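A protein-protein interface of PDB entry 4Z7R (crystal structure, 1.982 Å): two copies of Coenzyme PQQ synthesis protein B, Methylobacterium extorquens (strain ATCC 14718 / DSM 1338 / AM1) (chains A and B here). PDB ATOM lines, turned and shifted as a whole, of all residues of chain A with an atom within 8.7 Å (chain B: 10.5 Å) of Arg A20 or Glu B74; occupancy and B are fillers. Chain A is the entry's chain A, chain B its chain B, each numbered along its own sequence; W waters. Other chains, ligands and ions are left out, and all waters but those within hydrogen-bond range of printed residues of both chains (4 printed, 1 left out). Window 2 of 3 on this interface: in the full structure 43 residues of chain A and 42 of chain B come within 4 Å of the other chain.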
ATOM      1  N   PRO A  15      -7.591  -8.914   9.611  1.00  0.00           N
ATOM      2  CA  PRO A  15      -6.727 -10.051   9.280  1.00  0.00           C
ATOM      3  C   PRO A  15      -7.474 -11.377   9.339  1.00  0.00           C
ATOM      4  O   PRO A  15      -8.594 -11.437   9.848  1.00  0.00           O
ATOM      5  CB  PRO A  15      -5.652  -9.994  10.365  1.00  0.00           C
ATOM      6  CG  PRO A  15      -6.387  -9.454  11.553  1.00  0.00           C
ATOM      7  CD  PRO A  15      -7.369  -8.443  10.991  1.00  0.00           C
ATOM      8  N   GLN A  16      -6.852 -12.427   8.819  1.00  0.00           N
ATOM      9  CA  GLN A  16      -7.396 -13.770   8.945  1.00  0.00           C
ATOM     10  C   GLN A  16      -6.806 -14.413  10.197  1.00  0.00           C
ATOM     11  O   GLN A  16      -5.628 -14.220  10.500  1.00  0.00           O
ATOM     12  CB  GLN A  16      -7.093 -14.590   7.694  1.00  0.00           C
ATOM     13  CG  GLN A  16      -7.555 -16.031   7.741  1.00  0.00           C
ATOM     14  CD  GLN A  16      -7.367 -16.718   6.408  1.00  0.00           C
ATOM     15  OE1 GLN A  16      -7.907 -16.279   5.391  1.00  0.00           O
ATOM     16  NE2 GLN A  16      -6.575 -17.781   6.397  1.00  0.00           N
ATOM     17  N   TRP A  17      -7.631 -15.158  10.926  1.00  0.00           N
ATOM     18  CA  TRP A  17      -7.300 -15.574  12.290  1.00  0.00           C
ATOM     19  C   TRP A  17      -6.008 -16.376  12.404  1.00  0.00           C
ATOM     20  O   TRP A  17      -5.350 -16.347  13.442  1.00  0.00           O
ATOM     21  CB  TRP A  17      -8.451 -16.386  12.883  1.00  0.00           C
ATOM     22  CG  TRP A  17      -8.585 -17.761  12.320  1.00  0.00           C
ATOM     23  CD1 TRP A  17      -9.103 -18.107  11.102  1.00  0.00           C
ATOM     24  CD2 TRP A  17      -8.208 -18.987  12.959  1.00  0.00           C
ATOM     25  NE1 TRP A  17      -9.067 -19.473  10.946  1.00  0.00           N
ATOM     26  CE2 TRP A  17      -8.525 -20.035  12.072  1.00  0.00           C
ATOM     27  CE3 TRP A  17      -7.637 -19.300  14.197  1.00  0.00           C
ATOM     28  CZ2 TRP A  17      -8.282 -21.374  12.381  1.00  0.00           C
ATOM     29  CZ3 TRP A  17      -7.399 -20.628  14.504  1.00  0.00           C
ATOM     30  CH2 TRP A  17      -7.725 -21.648  13.601  1.00  0.00           C
ATOM     31  N   ASN A  18      -5.644 -17.089  11.343  1.00  0.00           N
ATOM     32  CA  ASN A  18      -4.421 -17.887  11.359  1.00  0.00           C
ATOM     33  C   ASN A  18      -3.403 -17.440  10.315  1.00  0.00           C
ATOM     34  O   ASN A  18      -2.565 -18.227   9.877  1.00  0.00           O
ATOM     35  CB  ASN A  18      -4.755 -19.365  11.143  1.00  0.00           C
ATOM     36  CG  ASN A  18      -5.281 -19.642   9.749  1.00  0.00           C
ATOM     37  OD1 ASN A  18      -5.845 -18.759   9.101  1.00  0.00           O
ATOM     38  ND2 ASN A  18      -5.093 -20.869   9.276  1.00  0.00           N
ATOM     39  N   CYS A  19      -3.476 -16.179   9.906  1.00  0.00           N
ATOM     40  CA  CYS A  19      -2.562 -15.688   8.883  1.00  0.00           C
ATOM     41  C   CYS A  19      -1.622 -14.611   9.399  1.00  0.00           C
ATOM     42  O   CYS A  19      -2.038 -13.701  10.114  1.00  0.00           O
ATOM     43  CB  CYS A  19      -3.341 -15.151   7.682  1.00  0.00           C
ATOM     44  SG  CYS A  19      -2.283 -14.734   6.281  1.00  0.00           S
ATOM     45  N   ARG A  20      -0.351 -14.726   9.025  1.00  0.00           N
ATOM     46  CA  ARG A  20       0.640 -13.704   9.335  1.00  0.00           C
ATOM     47  C   ARG A  20       1.367 -13.236   8.081  1.00  0.00           C
ATOM     48  O   ARG A  20       2.564 -12.950   8.127  1.00  0.00           O
ATOM     49  CB  ARG A  20       1.652 -14.220  10.361  1.00  0.00           C
ATOM     50  CG  ARG A  20       1.156 -14.161  11.789  1.00  0.00           C
ATOM     51  CD  ARG A  20       1.023 -12.726  12.261  1.00  0.00           C
ATOM     52  NE  ARG A  20       2.263 -12.222  12.840  1.00  0.00           N
ATOM     53  CZ  ARG A  20       2.327 -11.558  13.988  1.00  0.00           C
ATOM     54  NH1 ARG A  20       1.217 -11.316  14.673  1.00  0.00           N
ATOM     55  NH2 ARG A  20       3.495 -11.134  14.451  1.00  0.00           N
ATOM     56  N   CYS A  21       0.653 -13.168   6.959  1.00  0.00           N
ATOM     57  CA  CYS A  21       1.208 -12.549   5.757  1.00  0.00           C
ATOM     58  C   CYS A  21       1.515 -11.079   6.051  1.00  0.00           C
ATOM     59  O   CYS A  21       1.132 -10.559   7.097  1.00  0.00           O
ATOM     60  CB  CYS A  21       0.256 -12.701   4.559  1.00  0.00           C
ATOM     61  SG  CYS A  21      -1.149 -11.544   4.434  1.00  0.00           S
ATOM     62  N   SER A  22       2.207 -10.413   5.134  1.00  0.00           N
ATOM     63  CA  SER A  22       2.648  -9.041   5.368  1.00  0.00           C
ATOM     64  C   SER A  22       1.470  -8.087   5.577  1.00  0.00           C
ATOM     65  O   SER A  22       1.569  -7.125   6.338  1.00  0.00           O
ATOM     66  CB  SER A  22       3.512  -8.557   4.202  1.00  0.00           C
ATOM     67  OG  SER A  22       2.895  -8.842   2.960  1.00  0.00           O
ATOM     68  N   ILE A  23       0.352  -8.361   4.914  1.00  0.00           N
ATOM     69  CA  ILE A  23      -0.829  -7.516   5.047  1.00  0.00           C
ATOM     70  C   ILE A  23      -1.521  -7.729   6.394  1.00  0.00           C
ATOM     71  O   ILE A  23      -1.773  -6.768   7.127  1.00  0.00           O
ATOM     72  CB  ILE A  23      -1.822  -7.765   3.895  1.00  0.00           C
ATOM     73  CG1 ILE A  23      -1.215  -7.272   2.577  1.00  0.00           C
ATOM     74  CG2 ILE A  23      -3.142  -7.053   4.163  1.00  0.00           C
ATOM     75  CD1 ILE A  23      -1.841  -7.873   1.334  1.00  0.00           C
ATOM     76  N   CYS A  24      -1.817  -8.984   6.724  1.00  0.00           N
ATOM     77  CA  CYS A  24      -2.425  -9.306   8.013  1.00  0.00           C
ATOM     78  C   CYS A  24      -1.557  -8.848   9.180  1.00  0.00           C
ATOM     79  O   CYS A  24      -2.072  -8.347  10.178  1.00  0.00           O
ATOM     80  CB  CYS A  24      -2.696 -10.807   8.128  1.00  0.00           C
ATOM     81  SG  CYS A  24      -4.076 -11.388   7.120  1.00  0.00           S
ATOM     82  N   SER A  25      -0.243  -9.013   9.045  1.00  0.00           N
ATOM     83  CA  SER A  25       0.688  -8.624  10.099  1.00  0.00           C
ATOM     84  C   SER A  25       0.591  -7.133  10.402  1.00  0.00           C
ATOM     85  O   SER A  25       0.703  -6.717  11.555  1.00  0.00           O
ATOM     86  CB  SER A  25       2.122  -8.993   9.713  1.00  0.00           C
ATOM     87  OG  SER A  25       2.266 -10.398   9.615  1.00  0.00           O
ATOM     88  N   LEU A  26       0.387  -6.333   9.359  1.00  0.00           N
ATOM     89  CA  LEU A  26       0.168  -4.903   9.531  1.00  0.00           C
ATOM     90  C   LEU A  26      -1.105  -4.663  10.333  1.00  0.00           C
ATOM     91  O   LEU A  26      -1.130  -3.820  11.226  1.00  0.00           O
ATOM     92  CB  LEU A  26       0.092  -4.193   8.176  1.00  0.00           C
ATOM     93  CG  LEU A  26       1.423  -4.002   7.444  1.00  0.00           C
ATOM     94  CD1 LEU A  26       1.196  -3.611   5.993  1.00  0.00           C
ATOM     95  CD2 LEU A  26       2.279  -2.961   8.153  1.00  0.00           C
ATOM     96  N   ALA A  27      -2.157  -5.410  10.008  1.00  0.00           N
ATOM     97  CA  ALA A  27      -3.424  -5.308  10.722  1.00  0.00           C
ATOM     98  C   ALA A  27      -3.290  -5.740  12.182  1.00  0.00           C
ATOM     99  O   ALA A  27      -3.817  -5.079  13.078  1.00  0.00           O
ATOM    100  CB  ALA A  27      -4.495  -6.135  10.024  1.00  0.00           C
ATOM    101  N   TRP A  28      -2.588  -6.845  12.422  1.00  0.00           N
ATOM    102  CA  TRP A  28      -2.392  -7.332  13.787  1.00  0.00           C
ATOM    103  C   TRP A  28      -1.662  -6.300  14.646  1.00  0.00           C
ATOM    104  O   TRP A  28      -1.929  -6.169  15.841  1.00  0.00           O
ATOM    105  CB  TRP A  28      -1.606  -8.648  13.794  1.00  0.00           C
ATOM    106  CG  TRP A  28      -2.339  -9.840  13.239  1.00  0.00           C
ATOM    107  CD1 TRP A  28      -1.973 -10.594  12.161  1.00  0.00           C
ATOM    108  CD2 TRP A  28      -3.541 -10.433  13.751  1.00  0.00           C
ATOM    109  NE1 TRP A  28      -2.874 -11.610  11.962  1.00  0.00           N
ATOM    110  CE2 TRP A  28      -3.848 -11.533  12.922  1.00  0.00           C
ATOM    111  CE3 TRP A  28      -4.392 -10.136  14.822  1.00  0.00           C
ATOM    112  CZ2 TRP A  28      -4.970 -12.335  13.130  1.00  0.00           C
ATOM    113  CZ3 TRP A  28      -5.505 -10.938  15.029  1.00  0.00           C
ATOM    114  CH2 TRP A  28      -5.782 -12.024  14.190  1.00  0.00           C
ATOM    115  N   ALA A  29      -0.744  -5.567  14.025  1.00  0.00           N
ATOM    116  CA  ALA A  29       0.051  -4.563  14.725  1.00  0.00           C
ATOM    117  C   ALA A  29      -0.694  -3.242  14.880  1.00  0.00           C
ATOM    118  O   ALA A  29      -0.243  -2.350  15.597  1.00  0.00           O
ATOM    119  CB  ALA A  29       1.365  -4.337  13.998  1.00  0.00           C
ATOM    120  N   ALA A 228       2.139 -14.361  -1.551  1.00  0.00           N
ATOM    121  CA  ALA A 228       2.037 -13.961  -0.153  1.00  0.00           C
ATOM    122  C   ALA A 228       2.600 -15.039   0.764  1.00  0.00           C
ATOM    123  O   ALA A 228       2.855 -14.792   1.942  1.00  0.00           O
ATOM    124  CB  ALA A 228       0.590 -13.657   0.213  1.00  0.00           C
ATOM    125  N   GLY A 229       2.780 -16.238   0.218  1.00  0.00           N
ATOM    126  CA  GLY A 229       3.365 -17.338   0.961  1.00  0.00           C
ATOM    127  C   GLY A 229       2.411 -18.037   1.912  1.00  0.00           C
ATOM    128  O   GLY A 229       2.850 -18.703   2.848  1.00  0.00           O
ATOM    129  N   VAL A 230       1.109 -17.890   1.680  1.00  0.00           N
ATOM    130  CA  VAL A 230       0.118 -18.457   2.591  1.00  0.00           C
ATOM    131  C   VAL A 230      -0.611 -19.666   2.011  1.00  0.00           C
ATOM    132  O   VAL A 230      -1.311 -20.377   2.731  1.00  0.00           O
ATOM    133  CB  VAL A 230      -0.950 -17.416   2.988  1.00  0.00           C
ATOM    134  CG1 VAL A 230      -0.295 -16.143   3.487  1.00  0.00           C
ATOM    135  CG2 VAL A 230      -1.857 -17.114   1.808  1.00  0.00           C
ATOM    136  N   ASN A 268      -7.300 -11.204   2.127  1.00  0.00           N
ATOM    137  CA  ASN A 268      -6.267 -10.616   2.970  1.00  0.00           C
ATOM    138  C   ASN A 268      -4.906 -10.547   2.282  1.00  0.00           C
ATOM    139  O   ASN A 268      -4.033  -9.797   2.702  1.00  0.00           O
ATOM    140  CB  ASN A 268      -6.141 -11.399   4.280  1.00  0.00           C
ATOM    141  CG  ASN A 268      -5.583 -12.795   4.079  1.00  0.00           C
ATOM    142  OD1 ASN A 268      -4.365 -12.990   4.047  1.00  0.00           O
ATOM    143  ND2 ASN A 268      -6.470 -13.775   3.944  1.00  0.00           N
ATOM    144  N   THR A 269      -4.730 -11.338   1.227  1.00  0.00           N
ATOM    145  CA  THR A 269      -3.465 -11.393   0.501  1.00  0.00           C
ATOM    146  C   THR A 269      -3.363 -10.380  -0.642  1.00  0.00           C
ATOM    147  O   THR A 269      -2.371 -10.355  -1.368  1.00  0.00           O
ATOM    148  CB  THR A 269      -3.239 -12.796  -0.083  1.00  0.00           C
ATOM    149  OG1 THR A 269      -4.378 -13.164  -0.871  1.00  0.00           O
ATOM    150  CG2 THR A 269      -3.065 -13.815   1.032  1.00  0.00           C
ATOM    151  N   ILE B  64     -10.763 -13.469  18.786  1.00  0.00           N
ATOM    152  CA  ILE B  64      -9.361 -13.714  18.476  1.00  0.00           C
ATOM    153  C   ILE B  64      -8.649 -12.378  18.253  1.00  0.00           C
ATOM    154  O   ILE B  64      -7.565 -12.153  18.780  1.00  0.00           O
ATOM    155  CB  ILE B  64      -9.211 -14.635  17.242  1.00  0.00           C
ATOM    156  CG1 ILE B  64      -9.646 -16.059  17.600  1.00  0.00           C
ATOM    157  CG2 ILE B  64      -7.777 -14.637  16.727  1.00  0.00           C
ATOM    158  CD1 ILE B  64      -9.654 -17.017  16.432  1.00  0.00           C
ATOM    159  N   GLN B  65      -9.274 -11.479  17.499  1.00  0.00           N
ATOM    160  CA  GLN B  65      -8.680 -10.169  17.244  1.00  0.00           C
ATOM    161  C   GLN B  65      -8.474  -9.354  18.520  1.00  0.00           C
ATOM    162  O   GLN B  65      -7.434  -8.721  18.701  1.00  0.00           O
ATOM    163  CB  GLN B  65      -9.540  -9.371  16.261  1.00  0.00           C
ATOM    164  CG  GLN B  65      -9.502  -9.887  14.835  1.00  0.00           C
ATOM    165  CD  GLN B  65     -10.449  -9.131  13.930  1.00  0.00           C
ATOM    166  OE1 GLN B  65     -10.090  -8.100  13.359  1.00  0.00           O
ATOM    167  NE2 GLN B  65     -11.671  -9.633  13.800  1.00  0.00           N
ATOM    168  N   ASN B  67      -8.074 -10.239  21.559  1.00  0.00           N
ATOM    169  CA  ASN B  67      -7.222 -10.822  22.587  1.00  0.00           C
ATOM    170  C   ASN B  67      -5.892 -11.314  22.027  1.00  0.00           C
ATOM    171  O   ASN B  67      -5.830 -12.372  21.399  1.00  0.00           O
ATOM    172  CB  ASN B  67      -7.953 -11.966  23.291  1.00  0.00           C
ATOM    173  CG  ASN B  67      -9.190 -11.493  24.029  1.00  0.00           C
ATOM    174  OD1 ASN B  67      -9.111 -11.055  25.176  1.00  0.00           O
ATOM    175  ND2 ASN B  67     -10.336 -11.566  23.369  1.00  0.00           N
ATOM    176  N   PRO B  68      -4.825 -10.534  22.254  1.00  0.00           N
ATOM    177  CA  PRO B  68      -3.478 -10.769  21.721  1.00  0.00           C
ATOM    178  C   PRO B  68      -2.961 -12.181  21.985  1.00  0.00           C
ATOM    179  O   PRO B  68      -2.171 -12.693  21.193  1.00  0.00           O
ATOM    180  CB  PRO B  68      -2.634  -9.730  22.459  1.00  0.00           C
ATOM    181  CG  PRO B  68      -3.586  -8.613  22.704  1.00  0.00           C
ATOM    182  CD  PRO B  68      -4.876  -9.301  23.062  1.00  0.00           C
ATOM    183  N   GLN B  69      -3.401 -12.790  23.084  1.00  0.00           N
ATOM    184  CA  GLN B  69      -3.071 -14.177  23.384  1.00  0.00           C
ATOM    185  C   GLN B  69      -3.481 -15.115  22.246  1.00  0.00           C
ATOM    186  O   GLN B  69      -2.868 -16.163  22.052  1.00  0.00           O
ATOM    187  CB  GLN B  69      -3.738 -14.627  24.688  1.00  0.00           C
ATOM    188  CG  GLN B  69      -3.424 -13.764  25.903  1.00  0.00           C
ATOM    189  CD  GLN B  69      -4.438 -12.653  26.112  1.00  0.00           C
ATOM    190  OE1 GLN B  69      -5.115 -12.231  25.176  1.00  0.00           O
ATOM    191  NE2 GLN B  69      -4.550 -12.179  27.347  1.00  0.00           N
ATOM    192  N   MET B  70      -4.519 -14.733  21.504  1.00  0.00           N
ATOM    193  CA  MET B  70      -5.047 -15.562  20.421  1.00  0.00           C
ATOM    194  C   MET B  70      -4.418 -15.251  19.061  1.00  0.00           C
ATOM    195  O   MET B  70      -4.640 -15.977  18.092  1.00  0.00           O
ATOM    196  CB  MET B  70      -6.566 -15.404  20.323  1.00  0.00           C
ATOM    197  CG  MET B  70      -7.334 -15.776  21.587  1.00  0.00           C
ATOM    198  SD  MET B  70      -7.257 -17.535  22.003  1.00  0.00           S
ATOM    199  CE  MET B  70      -5.937 -17.569  23.218  1.00  0.00           C
ATOM    200  N   HIS B  71      -3.647 -14.171  18.985  1.00  0.00           N
ATOM    201  CA  HIS B  71      -3.060 -13.759  17.717  1.00  0.00           C
ATOM    202  C   HIS B  71      -2.090 -14.819  17.198  1.00  0.00           C
ATOM    203  O   HIS B  71      -1.316 -15.390  17.968  1.00  0.00           O
ATOM    204  CB  HIS B  71      -2.349 -12.410  17.862  1.00  0.00           C
ATOM    205  CG  HIS B  71      -3.281 -11.259  18.091  1.00  0.00           C
ATOM    206  ND1 HIS B  71      -2.855  -9.947  18.104  1.00  0.00           N
ATOM    207  CD2 HIS B  71      -4.617 -11.221  18.315  1.00  0.00           C
ATOM    208  CE1 HIS B  71      -3.886  -9.152  18.326  1.00  0.00           C
ATOM    209  NE2 HIS B  71      -4.968  -9.901  18.459  1.00  0.00           N
ATOM    210  N   PRO B  72      -2.132 -15.087  15.886  1.00  0.00           N
ATOM    211  CA  PRO B  72      -1.246 -16.080  15.269  1.00  0.00           C
ATOM    212  C   PRO B  72       0.222 -15.712  15.432  1.00  0.00           C
ATOM    213  O   PRO B  72       0.557 -14.526  15.486  1.00  0.00           O
ATOM    214  CB  PRO B  72      -1.654 -16.049  13.792  1.00  0.00           C
ATOM    215  CG  PRO B  72      -2.251 -14.696  13.596  1.00  0.00           C
ATOM    216  CD  PRO B  72      -2.954 -14.386  14.886  1.00  0.00           C
ATOM    217  N   ARG B  73       1.081 -16.721  15.520  1.00  0.00           N
ATOM    218  CA  ARG B  73       2.512 -16.491  15.648  1.00  0.00           C
ATOM    219  C   ARG B  73       3.124 -16.394  14.259  1.00  0.00           C
ATOM    220  O   ARG B  73       2.455 -16.672  13.267  1.00  0.00           O
ATOM    221  CB  ARG B  73       3.174 -17.611  16.457  1.00  0.00           C
ATOM    222  CG  ARG B  73       2.581 -17.798  17.847  1.00  0.00           C
ATOM    223  CD  ARG B  73       3.427 -18.728  18.702  1.00  0.00           C
ATOM    224  NE  ARG B  73       4.757 -18.182  18.955  1.00  0.00           N
ATOM    225  CZ  ARG B  73       5.075 -17.455  20.021  1.00  0.00           C
ATOM    226  NH1 ARG B  73       4.159 -17.188  20.943  1.00  0.00           N
ATOM    227  NH2 ARG B  73       6.309 -16.997  20.167  1.00  0.00           N
ATOM    228  N   GLU B  74       4.389 -15.994  14.195  1.00  0.00           N
ATOM    229  CA  GLU B  74       5.097 -15.861  12.926  1.00  0.00           C
ATOM    230  C   GLU B  74       5.065 -17.142  12.095  1.00  0.00           C
ATOM    231  O   GLU B  74       5.168 -18.244  12.630  1.00  0.00           O
ATOM    232  CB  GLU B  74       6.545 -15.437  13.174  1.00  0.00           C
ATOM    233  CG  GLU B  74       6.681 -14.042  13.760  1.00  0.00           C
ATOM    234  CD  GLU B  74       6.181 -12.963  12.820  1.00  0.00           C
ATOM    235  OE1 GLU B  74       6.293 -13.141  11.589  1.00  0.00           O
ATOM    236  OE2 GLU B  74       5.677 -11.932  13.314  1.00  0.00           O
ATOM    237  N   GLY B  75       4.913 -16.988  10.784  1.00  0.00           N
ATOM    238  CA  GLY B  75       4.961 -18.120   9.876  1.00  0.00           C
ATOM    239  C   GLY B  75       3.610 -18.602   9.386  1.00  0.00           C
ATOM    240  O   GLY B  75       2.591 -17.929   9.554  1.00  0.00           O
ATOM    241  N   LEU B  76       3.609 -19.782   8.775  1.00  0.00           N
ATOM    242  CA  LEU B  76       2.417 -20.333   8.136  1.00  0.00           C
ATOM    243  C   LEU B  76       1.608 -21.202   9.093  1.00  0.00           C
ATOM    244  O   LEU B  76       2.161 -22.076   9.762  1.00  0.00           O
ATOM    245  CB  LEU B  76       2.817 -21.142   6.900  1.00  0.00           C
ATOM    246  CG  LEU B  76       1.721 -21.663   5.972  1.00  0.00           C
ATOM    247  CD1 LEU B  76       0.789 -20.536   5.540  1.00  0.00           C
ATOM    248  CD2 LEU B  76       2.344 -22.350   4.762  1.00  0.00           C
ATOM    249  N   ARG B  77       0.303 -20.946   9.154  1.00  0.00           N
ATOM    250  CA  ARG B  77      -0.632 -21.754   9.937  1.00  0.00           C
ATOM    251  C   ARG B  77      -0.139 -21.978  11.366  1.00  0.00           C
ATOM    252  O   ARG B  77      -0.052 -23.113  11.839  1.00  0.00           O
ATOM    253  CB  ARG B  77      -0.878 -23.098   9.244  1.00  0.00           C
ATOM    254  CG  ARG B  77      -1.529 -22.972   7.869  1.00  0.00           C
ATOM    255  CD  ARG B  77      -1.867 -24.335   7.276  1.00  0.00           C
ATOM    256  NE  ARG B  77      -0.681 -25.082   6.864  1.00  0.00           N
ATOM    257  CZ  ARG B  77      -0.094 -24.964   5.677  1.00  0.00           C
ATOM    258  NH1 ARG B  77      -0.581 -24.126   4.774  1.00  0.00           N
ATOM    259  NH2 ARG B  77       0.981 -25.685   5.393  1.00  0.00           N
ATOM    260  N   HIS B  78       0.183 -20.884  12.047  1.00  0.00           N
ATOM    261  CA  HIS B  78       0.824 -20.961  13.353  1.00  0.00           C
ATOM    262  C   HIS B  78      -0.033 -20.280  14.415  1.00  0.00           C
ATOM    263  O   HIS B  78       0.268 -19.169  14.853  1.00  0.00           O
ATOM    264  CB  HIS B  78       2.212 -20.318  13.298  1.00  0.00           C
ATOM    265  CG  HIS B  78       3.114 -20.728  14.423  1.00  0.00           C
ATOM    266  ND1 HIS B  78       4.376 -20.199  14.594  1.00  0.00           N
ATOM    267  CD2 HIS B  78       2.943 -21.625  15.421  1.00  0.00           C
ATOM    268  CE1 HIS B  78       4.939 -20.745  15.657  1.00  0.00           C
ATOM    269  NE2 HIS B  78       4.092 -21.613  16.178  1.00  0.00           N
ATOM    270  N   SER B  79      -1.106 -20.952  14.821  1.00  0.00           N
ATOM    271  CA  SER B  79      -2.035 -20.386  15.793  1.00  0.00           C
ATOM    272  C   SER B  79      -1.769 -20.906  17.201  1.00  0.00           C
ATOM    273  O   SER B  79      -1.399 -22.067  17.383  1.00  0.00           O
ATOM    274  CB  SER B  79      -3.479 -20.694  15.391  1.00  0.00           C
ATOM    275  OG  SER B  79      -4.384 -20.288  16.403  1.00  0.00           O
ATOM    276  N   PRO B  80      -1.960 -20.044  18.208  1.00  0.00           N
ATOM    277  CA  PRO B  80      -1.806 -20.494  19.595  1.00  0.00           C
ATOM    278  C   PRO B  80      -2.941 -21.425  20.027  1.00  0.00           C
ATOM    279  O   PRO B  80      -2.807 -22.111  21.038  1.00  0.00           O
ATOM    280  CB  PRO B  80      -1.819 -19.189  20.401  1.00  0.00           C
ATOM    281  CG  PRO B  80      -2.412 -18.166  19.505  1.00  0.00           C
ATOM    282  CD  PRO B  80      -2.117 -18.583  18.100  1.00  0.00           C
ATOM    283  N   GLU B 102      -9.549 -22.414   7.781  1.00  0.00           N
ATOM    284  CA  GLU B 102      -8.540 -22.231   6.741  1.00  0.00           C
ATOM    285  C   GLU B 102      -7.302 -23.105   6.929  1.00  0.00           C
ATOM    286  O   GLU B 102      -6.189 -22.599   7.057  1.00  0.00           O
ATOM    287  CB  GLU B 102      -8.122 -20.761   6.659  1.00  0.00           C
ATOM    288  CG  GLU B 102      -9.200 -19.835   6.109  1.00  0.00           C
ATOM    289  CD  GLU B 102     -10.129 -19.314   7.188  1.00  0.00           C
ATOM    290  OE1 GLU B 102     -10.051 -19.807   8.333  1.00  0.00           O
ATOM    291  OE2 GLU B 102     -10.937 -18.410   6.892  1.00  0.00           O
ATOM    292  N   GLN B 104      -6.124 -24.891   9.320  1.00  0.00           N
ATOM    293  CA  GLN B 104      -5.411 -24.901  10.594  1.00  0.00           C
ATOM    294  C   GLN B 104      -5.625 -26.209  11.343  1.00  0.00           C
ATOM    295  O   GLN B 104      -6.758 -26.559  11.673  1.00  0.00           O
ATOM    296  CB  GLN B 104      -5.859 -23.735  11.476  1.00  0.00           C
ATOM    297  CG  GLN B 104      -5.014 -23.548  12.727  1.00  0.00           C
ATOM    298  CD  GLN B 104      -3.613 -23.074  12.410  1.00  0.00           C
ATOM    299  OE1 GLN B 104      -3.394 -22.383  11.417  1.00  0.00           O
ATOM    300  NE2 GLN B 104      -2.652 -23.447  13.249  1.00  0.00           N
HETATM  301  O   HOH W   1      -4.582 -17.531  15.909  1.00  0.00           O
HETATM  302  O   HOH W   2       4.806 -14.784   8.930  1.00  0.00           O
HETATM  303  O   HOH W   3       0.982 -16.659   7.796  1.00  0.00           O
HETATM  304  O   HOH W   4      -1.219 -18.927   7.719  1.00  0.00           O
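OE1 of Glu B102 sits at hydrogen-bond distance from NE1 of Trp A17, at 2.8 Å.
ND2 of Asn A18 is in hydrogen-bond range of O of Glu B102 (3.0 Å).
OE1 of Gln B104 is in hydrogen-bond range of ND2 of Asn A18.
O of Pro B72 sits at hydrogen-bond distance from NH1 of Arg A20.
The side-chain carboxylate of Glu B74 lies within salt-bridge range of the guanidinium group of Arg A20 (2.6 Å).
The backbone NH (N) of Gln A16 sits close to the side-chain sulfur (SG) of Cys A24 (3.4 Å).
The backbone carbonyl oxygen of Ile B64 sits close to a ring nitrogen (NE2) of His B71, at 3.5 Å.
O of Gln B65 is in hydrogen-bond range of NE2 of His B71 (2.7 Å).
The backbone carbonyl oxygen (O) of Glu B74 lies within hydrogen-bond range of a ring nitrogen (ND1) of His B78, at 2.9 Å.
The side-chain amide nitrogen of Gln B104 lies close to the backbone NH of Ser B79 (3.3 Å).
Glu B102 touches Gln A16 (CG to NE2, 3.3 Å).
Trp A17 touches Ile B64.
Trp A17 touches Pro B72 (O to CD, 3.4 Å).
CZ3 of Trp A17 touches OG of Ser B79, at 3.6 Å.
Trp A17 touches Gln B104 (CH2 to CG, 3.4 Å).
Gly B75 touches Arg A20 (O to CB, 3.9 Å).
Trp A28 touches His B71.
CZ2 of Trp A28 touches CD of Pro B72, 3.4 Å away.
Gly A229 touches Leu B76.
CD1 of Leu B76 touches O of Val A230, at 3.5 Å.
Cys A19 touches just one residue of chain B: Pro B72.
Arg A20 touches just these residues of chain B: Pro B72, Arg B73, Glu B74 and Gly B75.
No residue of chain B comes within 4 Å of Cys A21.
No residue of chain B comes within 4 Å of Cys A24.
No residue of chain B comes within 4 Å of Ser A25.
Of the printed residues of chain A, Gln B65 touches Pro A15 (3.6 Å) and Trp A28 (3.9 Å).
Of the printed residues of chain A, Pro B72 touches Trp A17, Cys A19, Arg A20 and Trp A28.
Gly B75 touches just one residue of chain A: Arg A20 (3.9 Å).
Of the printed residues of chain A, Ser B79 touches Trp A17.
Printed residues of chain A within 4 Å of Glu B102: Gln A16 (3.3 Å), Trp A17 (2.8 Å) and Asn A18 (3.0 Å).
The nearest residue of chain A that does not touch Glu B74 is Ser A25 (5.3 Å).
Of the 18 printed residues of chain B, 11 touch a printed residue of chain A.
Hydrophobic or aromatic side chains of chain B within 4 Å of the printed part of chain A: Ile B64, His B71, Pro B72 and Leu B76.
Along chain B the printed residues that touch a printed residue of chain A span positions 64 to 104.
Printed residues of chain A that touch a printed residue of chain B: Pro A15, Gln A16, Trp A17, Asn A18, Cys A19, Arg A20, Trp A28, Gly A229 and Val A230.
Hydrophobic or aromatic side chains of chain A within 4 Å of the printed part of chain B: Pro A15, Trp A17 and Trp A28.
Among the printed residues, Asp or Glu carboxylates within 4 Å of a Lys or Arg side-chain nitrogen of the other chain: Arg A20 with Glu B74 (2.6 Å).
No position is printed for both chains.
Of the 19 pairs that touch across the chains among the printed residues, none has its exchanged pair printed and touching as well.
Water W3 lies within hydrogen-bond range of the backbone NH (N) of Arg A20 and the backbone carbonyl oxygen (O) of Gly B75.
Water W1 lies within hydrogen-bond range of O of Met B70 (2.7 Å), OG of Ser B79 (2.8 Å) and O of Trp A17 (2.8 Å).
Water W2 lies within hydrogen-bond range of the backbone NH (N) of Gly B75 (2.9 Å), the backbone carbonyl oxygen (O) of Arg A20 (3.0 Å) and the side-chain carboxylate (OE1) of Glu B74 (3.5 Å).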
